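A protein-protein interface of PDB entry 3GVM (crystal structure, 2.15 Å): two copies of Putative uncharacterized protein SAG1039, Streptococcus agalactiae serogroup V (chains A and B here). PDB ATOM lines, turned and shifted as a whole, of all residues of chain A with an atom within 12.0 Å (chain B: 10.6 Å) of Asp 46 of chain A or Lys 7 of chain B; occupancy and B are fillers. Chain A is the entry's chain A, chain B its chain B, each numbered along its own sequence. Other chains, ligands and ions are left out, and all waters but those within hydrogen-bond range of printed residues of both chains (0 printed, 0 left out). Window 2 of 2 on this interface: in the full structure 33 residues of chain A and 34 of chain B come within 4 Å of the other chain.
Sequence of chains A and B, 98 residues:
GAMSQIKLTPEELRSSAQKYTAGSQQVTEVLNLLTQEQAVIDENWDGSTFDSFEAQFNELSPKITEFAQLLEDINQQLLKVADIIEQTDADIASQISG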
ATOM      1  N   GLU A  37      12.892 -15.206   3.555  1.00  0.00           N
ATOM      2  CA  GLU A  37      12.519 -15.656   4.901  1.00  0.00           C
ATOM      3  C   GLU A  37      12.601 -14.539   5.933  1.00  0.00           C
ATOM      4  O   GLU A  37      11.800 -14.500   6.868  1.00  0.00           O
ATOM      5  CB  GLU A  37      13.370 -16.834   5.387  1.00  0.00           C
ATOM      6  CG  GLU A  37      13.077 -18.145   4.709  1.00  0.00           C
ATOM      7  CD  GLU A  37      11.600 -18.523   4.725  1.00  0.00           C
ATOM      8  OE1 GLU A  37      11.040 -18.723   5.819  1.00  0.00           O
ATOM      9  OE2 GLU A  37      11.016 -18.649   3.630  1.00  0.00           O
ATOM     10  N   GLN A  38      13.592 -13.664   5.795  1.00  0.00           N
ATOM     11  CA  GLN A  38      13.728 -12.524   6.698  1.00  0.00           C
ATOM     12  C   GLN A  38      12.453 -11.664   6.649  1.00  0.00           C
ATOM     13  O   GLN A  38      11.941 -11.244   7.681  1.00  0.00           O
ATOM     14  CB  GLN A  38      14.950 -11.668   6.336  1.00  0.00           C
ATOM     15  CG  GLN A  38      16.306 -12.308   6.638  1.00  0.00           C
ATOM     16  CD  GLN A  38      16.651 -12.281   8.111  1.00  0.00           C
ATOM     17  OE1 GLN A  38      17.019 -11.234   8.657  1.00  0.00           O
ATOM     18  NE2 GLN A  38      16.539 -13.434   8.771  1.00  0.00           N
ATOM     19  N   ALA A  39      11.955 -11.420   5.440  1.00  0.00           N
ATOM     20  CA  ALA A  39      10.744 -10.636   5.239  1.00  0.00           C
ATOM     21  C   ALA A  39       9.537 -11.314   5.886  1.00  0.00           C
ATOM     22  O   ALA A  39       8.797 -10.684   6.637  1.00  0.00           O
ATOM     23  CB  ALA A  39      10.499 -10.412   3.761  1.00  0.00           C
ATOM     24  N   VAL A  40       9.350 -12.596   5.587  1.00  0.00           N
ATOM     25  CA  VAL A  40       8.302 -13.394   6.208  1.00  0.00           C
ATOM     26  C   VAL A  40       8.345 -13.274   7.729  1.00  0.00           C
ATOM     27  O   VAL A  40       7.320 -13.052   8.377  1.00  0.00           O
ATOM     28  CB  VAL A  40       8.419 -14.872   5.815  1.00  0.00           C
ATOM     29  CG1 VAL A  40       7.505 -15.739   6.683  1.00  0.00           C
ATOM     30  CG2 VAL A  40       8.096 -15.049   4.344  1.00  0.00           C
ATOM     31  N   ILE A  41       9.534 -13.413   8.299  1.00  0.00           N
ATOM     32  CA  ILE A  41       9.676 -13.317   9.743  1.00  0.00           C
ATOM     33  C   ILE A  41       9.347 -11.914  10.249  1.00  0.00           C
ATOM     34  O   ILE A  41       8.814 -11.747  11.343  1.00  0.00           O
ATOM     35  CB  ILE A  41      11.075 -13.706  10.202  1.00  0.00           C
ATOM     36  CG1 ILE A  41      11.292 -15.216  10.004  1.00  0.00           C
ATOM     37  CG2 ILE A  41      11.296 -13.283  11.657  1.00  0.00           C
ATOM     38  CD1 ILE A  41      12.676 -15.695  10.412  1.00  0.00           C
ATOM     39  N   ASP A  42       9.659 -10.906   9.444  1.00  0.00           N
ATOM     40  CA  ASP A  42       9.412  -9.523   9.829  1.00  0.00           C
ATOM     41  C   ASP A  42       7.907  -9.211   9.856  1.00  0.00           C
ATOM     42  O   ASP A  42       7.438  -8.464  10.711  1.00  0.00           O
ATOM     43  CB  ASP A  42      10.138  -8.585   8.864  1.00  0.00           C
ATOM     44  CG  ASP A  42      10.099  -7.137   9.309  1.00  0.00           C
ATOM     45  OD1 ASP A  42       9.783  -6.284   8.453  1.00  0.00           O
ATOM     46  OD2 ASP A  42      10.391  -6.848  10.494  1.00  0.00           O
ATOM     47  N   GLU A  43       7.165  -9.808   8.927  1.00  0.00           N
ATOM     48  CA  GLU A  43       5.744  -9.540   8.767  1.00  0.00           C
ATOM     49  C   GLU A  43       4.852 -10.393   9.667  1.00  0.00           C
ATOM     50  O   GLU A  43       3.734  -9.996   9.992  1.00  0.00           O
ATOM     51  CB  GLU A  43       5.334  -9.725   7.306  1.00  0.00           C
ATOM     52  CG  GLU A  43       5.866  -8.633   6.387  1.00  0.00           C
ATOM     53  CD  GLU A  43       5.810  -9.019   4.915  1.00  0.00           C
ATOM     54  OE1 GLU A  43       5.568 -10.212   4.615  1.00  0.00           O
ATOM     55  OE2 GLU A  43       6.015  -8.131   4.056  1.00  0.00           O
ATOM     56  N   ASN A  44       5.335 -11.564  10.063  1.00  0.00           N
ATOM     57  CA  ASN A  44       4.561 -12.434  10.945  1.00  0.00           C
ATOM     58  C   ASN A  44       5.077 -12.419  12.371  1.00  0.00           C
ATOM     59  O   ASN A  44       4.762 -13.303  13.171  1.00  0.00           O
ATOM     60  CB  ASN A  44       4.533 -13.862  10.419  1.00  0.00           C
ATOM     61  CG  ASN A  44       3.747 -13.988   9.147  1.00  0.00           C
ATOM     62  OD1 ASN A  44       2.622 -14.492   9.147  1.00  0.00           O
ATOM     63  ND2 ASN A  44       4.326 -13.525   8.047  1.00  0.00           N
ATOM     64  N   TRP A  45       5.879 -11.412  12.688  1.00  0.00           N
ATOM     65  CA  TRP A  45       6.392 -11.259  14.037  1.00  0.00           C
ATOM     66  C   TRP A  45       6.454  -9.782  14.389  1.00  0.00           C
ATOM     67  O   TRP A  45       7.532  -9.185  14.391  1.00  0.00           O
ATOM     68  CB  TRP A  45       7.786 -11.874  14.164  1.00  0.00           C
ATOM     69  CG  TRP A  45       8.244 -12.003  15.578  1.00  0.00           C
ATOM     70  CD1 TRP A  45       7.718 -11.370  16.666  1.00  0.00           C
ATOM     71  CD2 TRP A  45       9.338 -12.795  16.062  1.00  0.00           C
ATOM     72  NE1 TRP A  45       8.407 -11.731  17.800  1.00  0.00           N
ATOM     73  CE2 TRP A  45       9.409 -12.602  17.454  1.00  0.00           C
ATOM     74  CE3 TRP A  45      10.258 -13.655  15.454  1.00  0.00           C
ATOM     75  CZ2 TRP A  45      10.364 -13.233  18.250  1.00  0.00           C
ATOM     76  CZ3 TRP A  45      11.210 -14.284  16.249  1.00  0.00           C
ATOM     77  CH2 TRP A  45      11.251 -14.070  17.630  1.00  0.00           C
ATOM     78  N   ASP A  46       5.290  -9.196  14.671  1.00  0.00           N
ATOM     79  CA  ASP A  46       5.208  -7.797  15.075  1.00  0.00           C
ATOM     80  C   ASP A  46       6.092  -7.604  16.294  1.00  0.00           C
ATOM     81  O   ASP A  46       6.232  -8.508  17.117  1.00  0.00           O
ATOM     82  CB  ASP A  46       3.765  -7.412  15.406  1.00  0.00           C
ATOM     83  CG  ASP A  46       2.791  -7.785  14.303  1.00  0.00           C
ATOM     84  OD1 ASP A  46       1.588  -7.942  14.604  1.00  0.00           O
ATOM     85  OD2 ASP A  46       3.223  -7.930  13.136  1.00  0.00           O
ATOM     86  N   GLY A  47       6.698  -6.429  16.404  1.00  0.00           N
ATOM     87  CA  GLY A  47       7.622  -6.174  17.491  1.00  0.00           C
ATOM     88  C   GLY A  47       9.026  -5.889  16.999  1.00  0.00           C
ATOM     89  O   GLY A  47       9.248  -5.629  15.811  1.00  0.00           O
ATOM     90  N   SER A  48       9.981  -5.947  17.918  1.00  0.00           N
ATOM     91  CA  SER A  48      11.357  -5.590  17.614  1.00  0.00           C
ATOM     92  C   SER A  48      12.309  -6.620  18.208  1.00  0.00           C
ATOM     93  O   SER A  48      13.520  -6.398  18.288  1.00  0.00           O
ATOM     94  CB  SER A  48      11.666  -4.198  18.168  1.00  0.00           C
ATOM     95  OG  SER A  48      11.588  -4.187  19.586  1.00  0.00           O
ATOM     96  N   THR A  49      11.746  -7.747  18.629  1.00  0.00           N
ATOM     97  CA  THR A  49      12.526  -8.834  19.204  1.00  0.00           C
ATOM     98  C   THR A  49      13.561  -9.340  18.199  1.00  0.00           C
ATOM     99  O   THR A  49      14.621  -9.850  18.578  1.00  0.00           O
ATOM    100  CB  THR A  49      11.613 -10.019  19.598  1.00  0.00           C
ATOM    101  OG1 THR A  49      10.463  -9.534  20.303  1.00  0.00           O
ATOM    102  CG2 THR A  49      12.364 -11.019  20.465  1.00  0.00           C
ATOM    103  N   PHE A  50      13.245  -9.196  16.915  1.00  0.00           N
ATOM    104  CA  PHE A  50      14.077  -9.761  15.857  1.00  0.00           C
ATOM    105  C   PHE A  50      14.946  -8.702  15.169  1.00  0.00           C
ATOM    106  O   PHE A  50      15.617  -8.985  14.179  1.00  0.00           O
ATOM    107  CB  PHE A  50      13.186 -10.459  14.824  1.00  0.00           C
ATOM    108  CG  PHE A  50      13.895 -11.512  14.024  1.00  0.00           C
ATOM    109  CD1 PHE A  50      14.352 -12.671  14.638  1.00  0.00           C
ATOM    110  CD2 PHE A  50      14.094 -11.347  12.654  1.00  0.00           C
ATOM    111  CE1 PHE A  50      14.996 -13.648  13.907  1.00  0.00           C
ATOM    112  CE2 PHE A  50      14.750 -12.320  11.904  1.00  0.00           C
ATOM    113  CZ  PHE A  50      15.204 -13.471  12.530  1.00  0.00           C
ATOM    114  N   ASP A  51      14.925  -7.487  15.703  1.00  0.00           N
ATOM    115  CA  ASP A  51      15.584  -6.341  15.075  1.00  0.00           C
ATOM    116  C   ASP A  51      17.105  -6.467  14.947  1.00  0.00           C
ATOM    117  O   ASP A  51      17.686  -6.036  13.959  1.00  0.00           O
ATOM    118  CB  ASP A  51      15.227  -5.056  15.828  1.00  0.00           C
ATOM    119  CG  ASP A  51      13.871  -4.502  15.423  1.00  0.00           C
ATOM    120  OD1 ASP A  51      13.135  -5.198  14.686  1.00  0.00           O
ATOM    121  OD2 ASP A  51      13.551  -3.365  15.837  1.00  0.00           O
ATOM    122  N   SER A  52      17.743  -7.039  15.955  1.00  0.00           N
ATOM    123  CA  SER A  52      19.186  -7.200  15.951  1.00  0.00           C
ATOM    124  C   SER A  52      19.661  -8.170  14.858  1.00  0.00           C
ATOM    125  O   SER A  52      20.663  -7.920  14.189  1.00  0.00           O
ATOM    126  CB  SER A  52      19.658  -7.691  17.313  1.00  0.00           C
ATOM    127  OG  SER A  52      21.057  -7.928  17.306  1.00  0.00           O
ATOM    128  N   GLU A  54      17.944  -8.937  12.162  1.00  0.00           N
ATOM    129  CA  GLU A  54      17.614  -8.265  10.920  1.00  0.00           C
ATOM    130  C   GLU A  54      18.768  -7.360  10.474  1.00  0.00           C
ATOM    131  O   GLU A  54      19.098  -7.295   9.288  1.00  0.00           O
ATOM    132  CB  GLU A  54      16.342  -7.436  11.099  1.00  0.00           C
ATOM    133  CG  GLU A  54      15.843  -6.760   9.830  1.00  0.00           C
ATOM    134  CD  GLU A  54      14.779  -5.706  10.116  1.00  0.00           C
ATOM    135  OE1 GLU A  54      14.821  -5.107  11.217  1.00  0.00           O
ATOM    136  OE2 GLU A  54      13.906  -5.478   9.242  1.00  0.00           O
ATOM    137  N   GLN B   5       0.815 -11.801  18.878  1.00  0.00           N
ATOM    138  CA  GLN B   5       2.034 -11.092  18.457  1.00  0.00           C
ATOM    139  C   GLN B   5       2.882 -11.895  17.460  1.00  0.00           C
ATOM    140  O   GLN B   5       3.395 -11.349  16.463  1.00  0.00           O
ATOM    141  CB  GLN B   5       2.874 -10.699  19.677  1.00  0.00           C
ATOM    142  CG  GLN B   5       3.938  -9.638  19.397  1.00  0.00           C
ATOM    143  CD  GLN B   5       4.154  -8.711  20.588  1.00  0.00           C
ATOM    144  OE1 GLN B   5       3.352  -8.698  21.528  1.00  0.00           O
ATOM    145  NE2 GLN B   5       5.234  -7.928  20.552  1.00  0.00           N
ATOM    146  N   ILE B   6       3.031 -13.190  17.732  1.00  0.00           N
ATOM    147  CA  ILE B   6       3.744 -14.086  16.819  1.00  0.00           C
ATOM    148  C   ILE B   6       2.772 -14.939  16.009  1.00  0.00           C
ATOM    149  O   ILE B   6       2.202 -15.919  16.510  1.00  0.00           O
ATOM    150  CB  ILE B   6       4.735 -14.996  17.563  1.00  0.00           C
ATOM    151  CG1 ILE B   6       5.800 -14.146  18.256  1.00  0.00           C
ATOM    152  CG2 ILE B   6       5.382 -15.973  16.592  1.00  0.00           C
ATOM    153  CD1 ILE B   6       6.705 -14.933  19.184  1.00  0.00           C
ATOM    154  N   LYS B   7       2.591 -14.559  14.752  1.00  0.00           N
ATOM    155  CA  LYS B   7       1.632 -15.220  13.888  1.00  0.00           C
ATOM    156  C   LYS B   7       2.114 -16.581  13.403  1.00  0.00           C
ATOM    157  O   LYS B   7       1.305 -17.417  13.029  1.00  0.00           O
ATOM    158  CB  LYS B   7       1.288 -14.320  12.706  1.00  0.00           C
ATOM    159  CG  LYS B   7       0.906 -12.909  13.117  1.00  0.00           C
ATOM    160  CD  LYS B   7       0.463 -12.085  11.923  1.00  0.00           C
ATOM    161  CE  LYS B   7       0.212 -10.633  12.320  1.00  0.00           C
ATOM    162  NZ  LYS B   7       1.469  -9.955  12.749  1.00  0.00           N
ATOM    163  N   LEU B   8       3.426 -16.812  13.407  1.00  0.00           N
ATOM    164  CA  LEU B   8       3.966 -18.091  12.930  1.00  0.00           C
ATOM    165  C   LEU B   8       3.825 -19.204  13.958  1.00  0.00           C
ATOM    166  O   LEU B   8       4.251 -19.065  15.095  1.00  0.00           O
ATOM    167  CB  LEU B   8       5.438 -17.954  12.541  1.00  0.00           C
ATOM    168  CG  LEU B   8       5.769 -17.039  11.362  1.00  0.00           C
ATOM    169  CD1 LEU B   8       7.254 -17.118  11.034  1.00  0.00           C
ATOM    170  CD2 LEU B   8       4.942 -17.423  10.159  1.00  0.00           C
ATOM    171  N   THR B   9       3.255 -20.326  13.547  1.00  0.00           N
ATOM    172  CA  THR B   9       3.177 -21.481  14.432  1.00  0.00           C
ATOM    173  C   THR B   9       4.552 -22.116  14.643  1.00  0.00           C
ATOM    174  O   THR B   9       5.498 -21.835  13.904  1.00  0.00           O
ATOM    175  CB  THR B   9       2.236 -22.532  13.855  1.00  0.00           C
ATOM    176  OG1 THR B   9       2.808 -23.062  12.655  1.00  0.00           O
ATOM    177  CG2 THR B   9       0.885 -21.905  13.534  1.00  0.00           C
ATOM    178  N   PRO B  10       4.672 -22.971  15.664  1.00  0.00           N
ATOM    179  CA  PRO B  10       5.945 -23.666  15.894  1.00  0.00           C
ATOM    180  C   PRO B  10       6.407 -24.452  14.656  1.00  0.00           C
ATOM    181  O   PRO B  10       7.604 -24.542  14.385  1.00  0.00           O
ATOM    182  CB  PRO B  10       5.614 -24.622  17.040  1.00  0.00           C
ATOM    183  CG  PRO B  10       4.505 -23.904  17.800  1.00  0.00           C
ATOM    184  CD  PRO B  10       3.696 -23.204  16.748  1.00  0.00           C
ATOM    185  N   GLU B  11       5.462 -25.019  13.920  1.00  0.00           N
ATOM    186  CA  GLU B  11       5.800 -25.775  12.723  1.00  0.00           C
ATOM    187  C   GLU B  11       6.332 -24.853  11.631  1.00  0.00           C
ATOM    188  O   GLU B  11       7.286 -25.188  10.941  1.00  0.00           O
ATOM    189  CB  GLU B  11       4.592 -26.562  12.215  1.00  0.00           C
ATOM    190  CG  GLU B  11       4.927 -27.582  11.140  1.00  0.00           C
ATOM    191  CD  GLU B  11       3.683 -28.144  10.449  1.00  0.00           C
ATOM    192  OE1 GLU B  11       3.072 -27.419   9.629  1.00  0.00           O
ATOM    193  OE2 GLU B  11       3.322 -29.311  10.722  1.00  0.00           O
ATOM    194  N   GLU B  12       5.707 -23.693  11.466  1.00  0.00           N
ATOM    195  CA  GLU B  12       6.196 -22.717  10.502  1.00  0.00           C
ATOM    196  C   GLU B  12       7.572 -22.183  10.908  1.00  0.00           C
ATOM    197  O   GLU B  12       8.427 -21.919  10.067  1.00  0.00           O
ATOM    198  CB  GLU B  12       5.210 -21.567  10.369  1.00  0.00           C
ATOM    199  CG  GLU B  12       3.912 -21.957   9.682  1.00  0.00           C
ATOM    200  CD  GLU B  12       2.856 -20.869   9.800  1.00  0.00           C
ATOM    201  OE1 GLU B  12       2.758 -20.247  10.886  1.00  0.00           O
ATOM    202  OE2 GLU B  12       2.137 -20.629   8.805  1.00  0.00           O
ATOM    203  N   LEU B  13       7.779 -22.021  12.204  1.00  0.00           N
ATOM    204  CA  LEU B  13       9.050 -21.527  12.697  1.00  0.00           C
ATOM    205  C   LEU B  13      10.177 -22.527  12.409  1.00  0.00           C
ATOM    206  O   LEU B  13      11.299 -22.135  12.085  1.00  0.00           O
ATOM    207  CB  LEU B  13       8.964 -21.232  14.188  1.00  0.00           C
ATOM    208  CG  LEU B  13       8.195 -19.965  14.584  1.00  0.00           C
ATOM    209  CD1 LEU B  13       7.823 -20.031  16.060  1.00  0.00           C
ATOM    210  CD2 LEU B  13       9.022 -18.697  14.274  1.00  0.00           C
ATOM    211  N   VAL B  81      12.524 -20.645  20.169  1.00  0.00           N
ATOM    212  CA  VAL B  81      11.245 -19.958  20.251  1.00  0.00           C
ATOM    213  C   VAL B  81      10.106 -20.921  19.901  1.00  0.00           C
ATOM    214  O   VAL B  81       9.068 -20.927  20.568  1.00  0.00           O
ATOM    215  CB  VAL B  81      11.236 -18.695  19.371  1.00  0.00           C
ATOM    216  CG1 VAL B  81       9.836 -18.135  19.232  1.00  0.00           C
ATOM    217  CG2 VAL B  81      12.173 -17.642  19.965  1.00  0.00           C
ATOM    218  N   ILE B  85       6.886 -21.704  22.331  1.00  0.00           N
ATOM    219  CA  ILE B  85       5.513 -21.537  21.880  1.00  0.00           C
ATOM    220  C   ILE B  85       4.739 -22.848  21.875  1.00  0.00           C
ATOM    221  O   ILE B  85       3.553 -22.880  22.207  1.00  0.00           O
ATOM    222  CB  ILE B  85       5.431 -20.853  20.514  1.00  0.00           C
ATOM    223  CG1 ILE B  85       5.902 -19.400  20.640  1.00  0.00           C
ATOM    224  CG2 ILE B  85       4.009 -20.894  19.980  1.00  0.00           C
ATOM    225  CD1 ILE B  85       6.019 -18.673  19.321  1.00  0.00           C
ATOM    226  N   ASP B  89       1.245 -23.248  23.755  1.00  0.00           N
ATOM    227  CA  ASP B  89       0.019 -23.640  23.072  1.00  0.00           C
ATOM    228  C   ASP B  89      -0.614 -24.856  23.734  1.00  0.00           C
ATOM    229  O   ASP B  89      -1.845 -24.987  23.771  1.00  0.00           O
ATOM    230  CB  ASP B  89       0.288 -23.942  21.593  1.00  0.00           C
ATOM    231  CG  ASP B  89       0.543 -22.692  20.779  1.00  0.00           C
ATOM    232  OD1 ASP B  89       0.399 -21.582  21.331  1.00  0.00           O
ATOM    233  OD2 ASP B  89       0.886 -22.823  19.581  1.00  0.00           O
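The backbone carbonyl oxygen of Asn 44 of chain A sits at hydrogen-bond distance from the backbone NH of Lys 7 of chain B (3.0 Å).
N of Asp 46 of chain A lies within hydrogen-bond range of O of Gln 5 of chain B (3.4 Å).
The side-chain carboxylate (OD2) of Asp 46 of chain A lies within salt-bridge range of the side-chain amino group (NZ) of Lys 7 of chain B (2.7 Å).
The backbone carbonyl oxygen of Val 40 of chain A is in hydrogen-bond range of the side-chain amide nitrogen of Asn 44 of chain A, 3.0 Å away.
NZ of Lys 7 of chain B touches O of Glu 43 of chain A, 3.6 Å away.
Ile 6 of chain B touches Asn 44 of chain A.
Leu 8 of chain B touches Asn 44 of chain A (CG to CB, 3.5 Å).
CA of Trp 45 of chain A touches O of Gln 5 of chain B, 3.9 Å away.
Ile 6 of chain B touches Trp 45 of chain A.
Printed residues of chain B within 4 Å of Glu 43 of chain A: Lys 7 (3.6 Å).
Asn 44 of chain A touches three residues of chain B.
Of the printed residues of chain B, Trp 45 of chain A touches Gln 5 (3.9 Å) and Ile 6 (3.6 Å).
Asp 46 of chain A touches just these residues of chain B: Gln 5 and Lys 7.
No residue of chain B comes within 4 Å of Gly 47 of chain A.
Gln 5 of chain B touches just these residues of chain A: Trp 45 (3.9 Å) and Asp 46 (3.4 Å).
Ile 6 of chain B touches two residues of chain A.
Of chain A, only Glu 43, Asn 44 and Asp 46 come within 4 Å of Lys 7 of chain B.
Leu 8 of chain B touches just one residue of chain A: Asn 44 (3.5 Å).
No residue of chain A comes within 4 Å of Thr 9 of chain B.
Asp 89 of chain B touches none of the printed residues of chain A.
The nearest residue of chain A that does not touch Lys 7 of chain B is Trp 45 of chain A (4.6 Å).
Of the 12 printed residues of chain B, 4 touch a printed residue of chain A.
Printed residues of chain B that touch a printed residue of chain A: Gln 5, Ile 6, Lys 7 and Leu 8.
Among the printed residues, 8 pairs touch across the chains.
No position is printed for both chains.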
